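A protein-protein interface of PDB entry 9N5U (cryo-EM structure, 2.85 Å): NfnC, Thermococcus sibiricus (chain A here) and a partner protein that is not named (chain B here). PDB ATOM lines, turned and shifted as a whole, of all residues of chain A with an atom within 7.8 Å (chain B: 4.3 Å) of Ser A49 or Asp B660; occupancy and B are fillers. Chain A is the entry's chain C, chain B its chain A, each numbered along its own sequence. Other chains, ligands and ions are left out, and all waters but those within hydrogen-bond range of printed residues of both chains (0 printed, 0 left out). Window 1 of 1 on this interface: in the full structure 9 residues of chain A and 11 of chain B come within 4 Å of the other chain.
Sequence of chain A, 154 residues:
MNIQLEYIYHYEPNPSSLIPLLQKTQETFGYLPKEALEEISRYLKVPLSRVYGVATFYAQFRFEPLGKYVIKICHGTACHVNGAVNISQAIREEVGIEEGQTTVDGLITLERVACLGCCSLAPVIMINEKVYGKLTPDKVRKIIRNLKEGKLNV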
ATOM      1  N   SER A  41      -6.690   4.487  11.442  1.00  0.00           N
ATOM      2  CA  SER A  41      -7.744   5.483  11.585  1.00  0.00           C
ATOM      3  C   SER A  41      -7.327   6.829  11.015  1.00  0.00           C
ATOM      4  O   SER A  41      -8.163   7.566  10.486  1.00  0.00           O
ATOM      5  CB  SER A  41      -8.124   5.627  13.056  1.00  0.00           C
ATOM      6  OG  SER A  41      -9.026   6.698  13.249  1.00  0.00           O
ATOM      7  N   VAL A  46     -11.135   7.481   9.295  1.00  0.00           N
ATOM      8  CA  VAL A  46     -12.301   6.916   9.965  1.00  0.00           C
ATOM      9  C   VAL A  46     -12.099   7.094  11.464  1.00  0.00           C
ATOM     10  O   VAL A  46     -10.952   7.154  11.927  1.00  0.00           O
ATOM     11  CB  VAL A  46     -12.508   5.439   9.596  1.00  0.00           C
ATOM     12  CG1 VAL A  46     -12.955   5.311   8.154  1.00  0.00           C
ATOM     13  CG2 VAL A  46     -11.238   4.657   9.826  1.00  0.00           C
ATOM     14  N   PRO A  47     -13.167   7.218  12.250  1.00  0.00           N
ATOM     15  CA  PRO A  47     -13.000   7.309  13.701  1.00  0.00           C
ATOM     16  C   PRO A  47     -12.390   6.039  14.271  1.00  0.00           C
ATOM     17  O   PRO A  47     -12.588   4.939  13.754  1.00  0.00           O
ATOM     18  CB  PRO A  47     -14.429   7.522  14.210  1.00  0.00           C
ATOM     19  CG  PRO A  47     -15.144   8.120  13.061  1.00  0.00           C
ATOM     20  CD  PRO A  47     -14.555   7.484  11.842  1.00  0.00           C
ATOM     21  N   LEU A  48     -11.621   6.212  15.343  1.00  0.00           N
ATOM     22  CA  LEU A  48     -11.007   5.068  16.000  1.00  0.00           C
ATOM     23  C   LEU A  48     -12.054   4.180  16.659  1.00  0.00           C
ATOM     24  O   LEU A  48     -11.843   2.970  16.801  1.00  0.00           O
ATOM     25  CB  LEU A  48      -9.974   5.555  17.014  1.00  0.00           C
ATOM     26  CG  LEU A  48      -8.916   4.574  17.509  1.00  0.00           C
ATOM     27  CD1 LEU A  48      -8.235   3.891  16.347  1.00  0.00           C
ATOM     28  CD2 LEU A  48      -7.898   5.308  18.354  1.00  0.00           C
ATOM     29  N   SER A  49     -13.193   4.759  17.047  1.00  0.00           N
ATOM     30  CA  SER A  49     -14.289   3.960  17.580  1.00  0.00           C
ATOM     31  C   SER A  49     -14.905   3.073  16.504  1.00  0.00           C
ATOM     32  O   SER A  49     -15.306   1.941  16.785  1.00  0.00           O
ATOM     33  CB  SER A  49     -15.342   4.872  18.209  1.00  0.00           C
ATOM     34  OG  SER A  49     -15.620   5.983  17.381  1.00  0.00           O
ATOM     35  N   ARG A  50     -14.983   3.567  15.266  1.00  0.00           N
ATOM     36  CA  ARG A  50     -15.461   2.736  14.162  1.00  0.00           C
ATOM     37  C   ARG A  50     -14.504   1.582  13.886  1.00  0.00           C
ATOM     38  O   ARG A  50     -14.936   0.446  13.647  1.00  0.00           O
ATOM     39  CB  ARG A  50     -15.645   3.592  12.911  1.00  0.00           C
ATOM     40  CG  ARG A  50     -16.670   3.064  11.929  1.00  0.00           C
ATOM     41  CD  ARG A  50     -18.067   3.149  12.507  1.00  0.00           C
ATOM     42  NE  ARG A  50     -19.035   3.649  11.540  1.00  0.00           N
ATOM     43  CZ  ARG A  50     -20.312   3.874  11.809  1.00  0.00           C
ATOM     44  NH1 ARG A  50     -20.816   3.638  13.008  1.00  0.00           N
ATOM     45  NH2 ARG A  50     -21.104   4.348  10.854  1.00  0.00           N
ATOM     46  N   VAL A  51     -13.199   1.863  13.923  1.00  0.00           N
ATOM     47  CA  VAL A  51     -12.189   0.827  13.738  1.00  0.00           C
ATOM     48  C   VAL A  51     -12.305  -0.228  14.826  1.00  0.00           C
ATOM     49  O   VAL A  51     -12.239  -1.434  14.556  1.00  0.00           O
ATOM     50  CB  VAL A  51     -10.785   1.456  13.715  1.00  0.00           C
ATOM     51  CG1 VAL A  51      -9.724   0.383  13.657  1.00  0.00           C
ATOM     52  CG2 VAL A  51     -10.650   2.393  12.543  1.00  0.00           C
ATOM     53  N   TYR A  52     -12.496   0.205  16.072  1.00  0.00           N
ATOM     54  CA  TYR A  52     -12.592  -0.757  17.161  1.00  0.00           C
ATOM     55  C   TYR A  52     -13.894  -1.548  17.097  1.00  0.00           C
ATOM     56  O   TYR A  52     -13.908  -2.739  17.414  1.00  0.00           O
ATOM     57  CB  TYR A  52     -12.432  -0.048  18.500  1.00  0.00           C
ATOM     58  CG  TYR A  52     -10.996  -0.023  18.962  1.00  0.00           C
ATOM     59  CD1 TYR A  52     -10.459  -1.088  19.667  1.00  0.00           C
ATOM     60  CD2 TYR A  52     -10.169   1.050  18.671  1.00  0.00           C
ATOM     61  CE1 TYR A  52      -9.149  -1.077  20.084  1.00  0.00           C
ATOM     62  CE2 TYR A  52      -8.856   1.070  19.086  1.00  0.00           C
ATOM     63  CZ  TYR A  52      -8.352   0.004  19.794  1.00  0.00           C
ATOM     64  OH  TYR A  52      -7.045   0.013  20.209  1.00  0.00           O
ATOM     65  N   GLY A  53     -14.988  -0.918  16.666  1.00  0.00           N
ATOM     66  CA  GLY A  53     -16.231  -1.655  16.499  1.00  0.00           C
ATOM     67  C   GLY A  53     -16.139  -2.725  15.429  1.00  0.00           C
ATOM     68  O   GLY A  53     -16.600  -3.857  15.621  1.00  0.00           O
ATOM     69  N   VAL A  54     -15.528  -2.389  14.290  1.00  0.00           N
ATOM     70  CA  VAL A  54     -15.322  -3.385  13.243  1.00  0.00           C
ATOM     71  C   VAL A  54     -14.396  -4.493  13.731  1.00  0.00           C
ATOM     72  O   VAL A  54     -14.657  -5.680  13.506  1.00  0.00           O
ATOM     73  CB  VAL A  54     -14.789  -2.714  11.964  1.00  0.00           C
ATOM     74  CG1 VAL A  54     -14.399  -3.756  10.940  1.00  0.00           C
ATOM     75  CG2 VAL A  54     -15.836  -1.787  11.387  1.00  0.00           C
ATOM     76  N   ALA A  55     -13.315  -4.130  14.423  1.00  0.00           N
ATOM     77  CA  ALA A  55     -12.351  -5.126  14.879  1.00  0.00           C
ATOM     78  C   ALA A  55     -12.935  -6.047  15.944  1.00  0.00           C
ATOM     79  O   ALA A  55     -12.548  -7.217  16.025  1.00  0.00           O
ATOM     80  CB  ALA A  55     -11.097  -4.433  15.406  1.00  0.00           C
ATOM     81  N   THR A  56     -13.845  -5.543  16.776  1.00  0.00           N
ATOM     82  CA  THR A  56     -14.462  -6.384  17.789  1.00  0.00           C
ATOM     83  C   THR A  56     -15.656  -7.164  17.257  1.00  0.00           C
ATOM     84  O   THR A  56     -16.088  -8.120  17.911  1.00  0.00           O
ATOM     85  CB  THR A  56     -14.887  -5.541  18.993  1.00  0.00           C
ATOM     86  OG1 THR A  56     -15.698  -4.444  18.557  1.00  0.00           O
ATOM     87  CG2 THR A  56     -13.669  -5.007  19.719  1.00  0.00           C
ATOM     88  N   VAL B 647     -25.061   6.408  18.200  1.00  0.00           N
ATOM     89  CA  VAL B 647     -24.064   6.047  17.196  1.00  0.00           C
ATOM     90  C   VAL B 647     -24.396   6.695  15.860  1.00  0.00           C
ATOM     91  O   VAL B 647     -23.520   7.254  15.187  1.00  0.00           O
ATOM     92  CB  VAL B 647     -23.968   4.517  17.078  1.00  0.00           C
ATOM     93  CG1 VAL B 647     -23.005   4.126  15.981  1.00  0.00           C
ATOM     94  CG2 VAL B 647     -23.542   3.921  18.396  1.00  0.00           C
ATOM     95  N   HIS B 651     -21.896   9.555  14.307  1.00  0.00           N
ATOM     96  CA  HIS B 651     -21.134   9.168  13.128  1.00  0.00           C
ATOM     97  C   HIS B 651     -21.681   9.727  11.822  1.00  0.00           C
ATOM     98  O   HIS B 651     -20.900   9.947  10.893  1.00  0.00           O
ATOM     99  CB  HIS B 651     -21.051   7.642  13.028  1.00  0.00           C
ATOM    100  CG  HIS B 651     -20.017   7.037  13.926  1.00  0.00           C
ATOM    101  ND1 HIS B 651     -18.667   7.134  13.674  1.00  0.00           N
ATOM    102  CD2 HIS B 651     -20.136   6.334  15.077  1.00  0.00           C
ATOM    103  CE1 HIS B 651     -17.997   6.510  14.626  1.00  0.00           C
ATOM    104  NE2 HIS B 651     -18.865   6.021  15.492  1.00  0.00           N
ATOM    105  N   GLY B 657     -17.704  10.721  15.976  1.00  0.00           N
ATOM    106  CA  GLY B 657     -17.398   9.354  16.346  1.00  0.00           C
ATOM    107  C   GLY B 657     -17.027   9.166  17.801  1.00  0.00           C
ATOM    108  O   GLY B 657     -16.035   8.504  18.111  1.00  0.00           O
ATOM    109  N   VAL B 659     -18.786   7.554  20.182  1.00  0.00           N
ATOM    110  CA  VAL B 659     -19.099   6.197  20.599  1.00  0.00           C
ATOM    111  C   VAL B 659     -19.406   5.360  19.367  1.00  0.00           C
ATOM    112  O   VAL B 659     -19.672   5.879  18.282  1.00  0.00           O
ATOM    113  CB  VAL B 659     -20.283   6.151  21.589  1.00  0.00           C
ATOM    114  CG1 VAL B 659     -19.900   6.791  22.906  1.00  0.00           C
ATOM    115  CG2 VAL B 659     -21.500   6.836  20.997  1.00  0.00           C
ATOM    116  N   ASP B 660     -19.349   4.046  19.546  1.00  0.00           N
ATOM    117  CA  ASP B 660     -19.727   3.120  18.491  1.00  0.00           C
ATOM    118  C   ASP B 660     -20.113   1.794  19.124  1.00  0.00           C
ATOM    119  O   ASP B 660     -19.825   1.536  20.296  1.00  0.00           O
ATOM    120  CB  ASP B 660     -18.597   2.926  17.475  1.00  0.00           C
ATOM    121  CG  ASP B 660     -19.074   2.283  16.188  1.00  0.00           C
ATOM    122  OD1 ASP B 660     -20.287   2.317  15.920  1.00  0.00           O
ATOM    123  OD2 ASP B 660     -18.240   1.730  15.451  1.00  0.00           O
ATOM    124  N   TYR B 661     -20.800   0.970  18.336  1.00  0.00           N
ATOM    125  CA  TYR B 661     -21.093  -0.397  18.737  1.00  0.00           C
ATOM    126  C   TYR B 661     -19.801  -1.159  18.989  1.00  0.00           C
ATOM    127  O   TYR B 661     -18.859  -1.092  18.198  1.00  0.00           O
ATOM    128  CB  TYR B 661     -21.889  -1.110  17.647  1.00  0.00           C
ATOM    129  CG  TYR B 661     -23.366  -0.806  17.579  1.00  0.00           C
ATOM    130  CD1 TYR B 661     -24.263  -1.458  18.407  1.00  0.00           C
ATOM    131  CD2 TYR B 661     -23.868   0.090  16.648  1.00  0.00           C
ATOM    132  CE1 TYR B 661     -25.612  -1.207  18.331  1.00  0.00           C
ATOM    133  CE2 TYR B 661     -25.220   0.347  16.566  1.00  0.00           C
ATOM    134  CZ  TYR B 661     -26.086  -0.304  17.413  1.00  0.00           C
ATOM    135  OH  TYR B 661     -27.433  -0.061  17.342  1.00  0.00           O
ATOM    136  N   LEU B 662     -19.760  -1.893  20.091  1.00  0.00           N
ATOM    137  CA  LEU B 662     -18.622  -2.740  20.406  1.00  0.00           C
ATOM    138  C   LEU B 662     -19.106  -4.161  20.638  1.00  0.00           C
ATOM    139  O   LEU B 662     -20.159  -4.375  21.242  1.00  0.00           O
ATOM    140  CB  LEU B 662     -17.864  -2.230  21.635  1.00  0.00           C
ATOM    141  CG  LEU B 662     -17.254  -0.833  21.536  1.00  0.00           C
ATOM    142  CD1 LEU B 662     -16.648  -0.437  22.864  1.00  0.00           C
ATOM    143  CD2 LEU B 662     -16.210  -0.764  20.440  1.00  0.00           C
ATOM    144  N   TYR B 669     -22.316  -3.457  23.355  1.00  0.00           N
ATOM    145  CA  TYR B 669     -22.551  -2.247  24.126  1.00  0.00           C
ATOM    146  C   TYR B 669     -22.015  -1.055  23.348  1.00  0.00           C
ATOM    147  O   TYR B 669     -21.436  -1.195  22.269  1.00  0.00           O
ATOM    148  CB  TYR B 669     -21.939  -2.345  25.528  1.00  0.00           C
ATOM    149  CG  TYR B 669     -20.432  -2.313  25.600  1.00  0.00           C
ATOM    150  CD1 TYR B 669     -19.685  -3.464  25.415  1.00  0.00           C
ATOM    151  CD2 TYR B 669     -19.758  -1.140  25.896  1.00  0.00           C
ATOM    152  CE1 TYR B 669     -18.314  -3.440  25.497  1.00  0.00           C
ATOM    153  CE2 TYR B 669     -18.387  -1.107  25.980  1.00  0.00           C
ATOM    154  CZ  TYR B 669     -17.670  -2.259  25.781  1.00  0.00           C
ATOM    155  OH  TYR B 669     -16.301  -2.227  25.864  1.00  0.00           O
ATOM    156  N   ILE B 670     -22.235   0.128  23.904  1.00  0.00           N
ATOM    157  CA  ILE B 670     -21.864   1.390  23.286  1.00  0.00           C
ATOM    158  C   ILE B 670     -20.730   1.995  24.098  1.00  0.00           C
ATOM    159  O   ILE B 670     -20.767   1.991  25.332  1.00  0.00           O
ATOM    160  CB  ILE B 670     -23.068   2.349  23.212  1.00  0.00           C
ATOM    161  CG1 ILE B 670     -24.264   1.664  22.546  1.00  0.00           C
ATOM    162  CG2 ILE B 670     -22.709   3.611  22.474  1.00  0.00           C
ATOM    163  CD1 ILE B 670     -24.128   1.478  21.064  1.00  0.00           C
ATOM    164  N   GLY B 671     -19.711   2.487  23.409  1.00  0.00           N
ATOM    165  CA  GLY B 671     -18.606   3.110  24.088  1.00  0.00           C
ATOM    166  C   GLY B 671     -17.551   3.634  23.144  1.00  0.00           C
ATOM    167  O   GLY B 671     -17.564   3.367  21.940  1.00  0.00           O
ATOM    168  N   GLN B 673     -13.425   4.032  21.868  1.00  0.00           N
ATOM    169  CA  GLN B 673     -12.456   2.989  21.571  1.00  0.00           C
ATOM    170  C   GLN B 673     -11.977   2.343  22.863  1.00  0.00           C
ATOM    171  O   GLN B 673     -11.916   2.980  23.917  1.00  0.00           O
ATOM    172  CB  GLN B 673     -11.272   3.551  20.782  1.00  0.00           C
ATOM    173  CG  GLN B 673     -10.430   4.571  21.509  1.00  0.00           C
ATOM    174  CD  GLN B 673     -10.816   5.984  21.156  1.00  0.00           C
ATOM    175  OE1 GLN B 673     -11.971   6.263  20.848  1.00  0.00           O
ATOM    176  NE2 GLN B 673      -9.847   6.885  21.186  1.00  0.00           N
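A ring nitrogen (NE2) of His B651 sits at hydrogen-bond distance from the backbone carbonyl oxygen (O) of Val B659 (2.9 Å). The backbone NH (N) of Asp B660 lies within hydrogen-bond range of the backbone carbonyl oxygen (O) of Gly B671. The backbone NH (N) of Leu B662 lies within hydrogen-bond range of the backbone carbonyl oxygen (O) of Tyr B669 (2.8 Å). N of Leu A48 lies within hydrogen-bond range of OG of Ser A41 (3.4 Å). O of Tyr A52 sits at hydrogen-bond distance from OG1 of Thr A56 (2.7 Å). O of Gly A53 sits at hydrogen-bond distance from OG1 of Thr A56 (3.1 Å).
Among the printed residues, merely in contact across the chains: Gly A53 with Tyr B661, Tyr A52 with Gln B673, Arg A50 with His B651, Pro A47 with His B651, Ser A49 with His B651, Arg A50 with Val B647, Leu A48 with Gln B673, Thr A56 with Leu B662 and Gly A53 with Leu B662.
Hydrophobic or aromatic side chains of chain A within 4 Å of the printed part of chain B: Pro A47, Leu A48 and Tyr A52. Of the 11 printed residues of chain B, 7 touch a printed residue of chain A. Among the printed residues, 12 pairs touch across the chains.
OG of Ser A49 is in hydrogen-bond range of O of Gly B657 (2.7 Å). OD1 of Asp B660 lies within salt-bridge range of NH1 of Arg A50 (3.2 Å). The backbone carbonyl oxygen (O) of Ser A49 lies close to the side-chain carboxylate (OD2) of Asp B660, 3.2 Å away.
Ser A49 touches just these residues of chain B: His B651, Gly B657 and Asp B660. Printed residues of chain B within 4 Å of Tyr A52: Gln B673 (3.5 Å). Of the printed residues of chain B, Thr A56 touches Leu B662. Of the printed residues of chain A, Val B647 touches Arg A50. Of the printed residues of chain A, Gly B657 touches Ser A49 (2.7 Å). Asp B660 touches just these residues of chain A: Ser A49 (3.2 Å) and Arg A50 (3.2 Å). Gly B671 touches none of the printed residues of chain A. Of the printed residues of chain A, Gln B673 touches Leu A48 and Tyr A52. The nearest residue of chain B that does not touch Ser A49 is Val B659 (4.2 Å). The nearest residue of chain A that does not touch Asp B660 is Gly A53 (4.1 Å).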
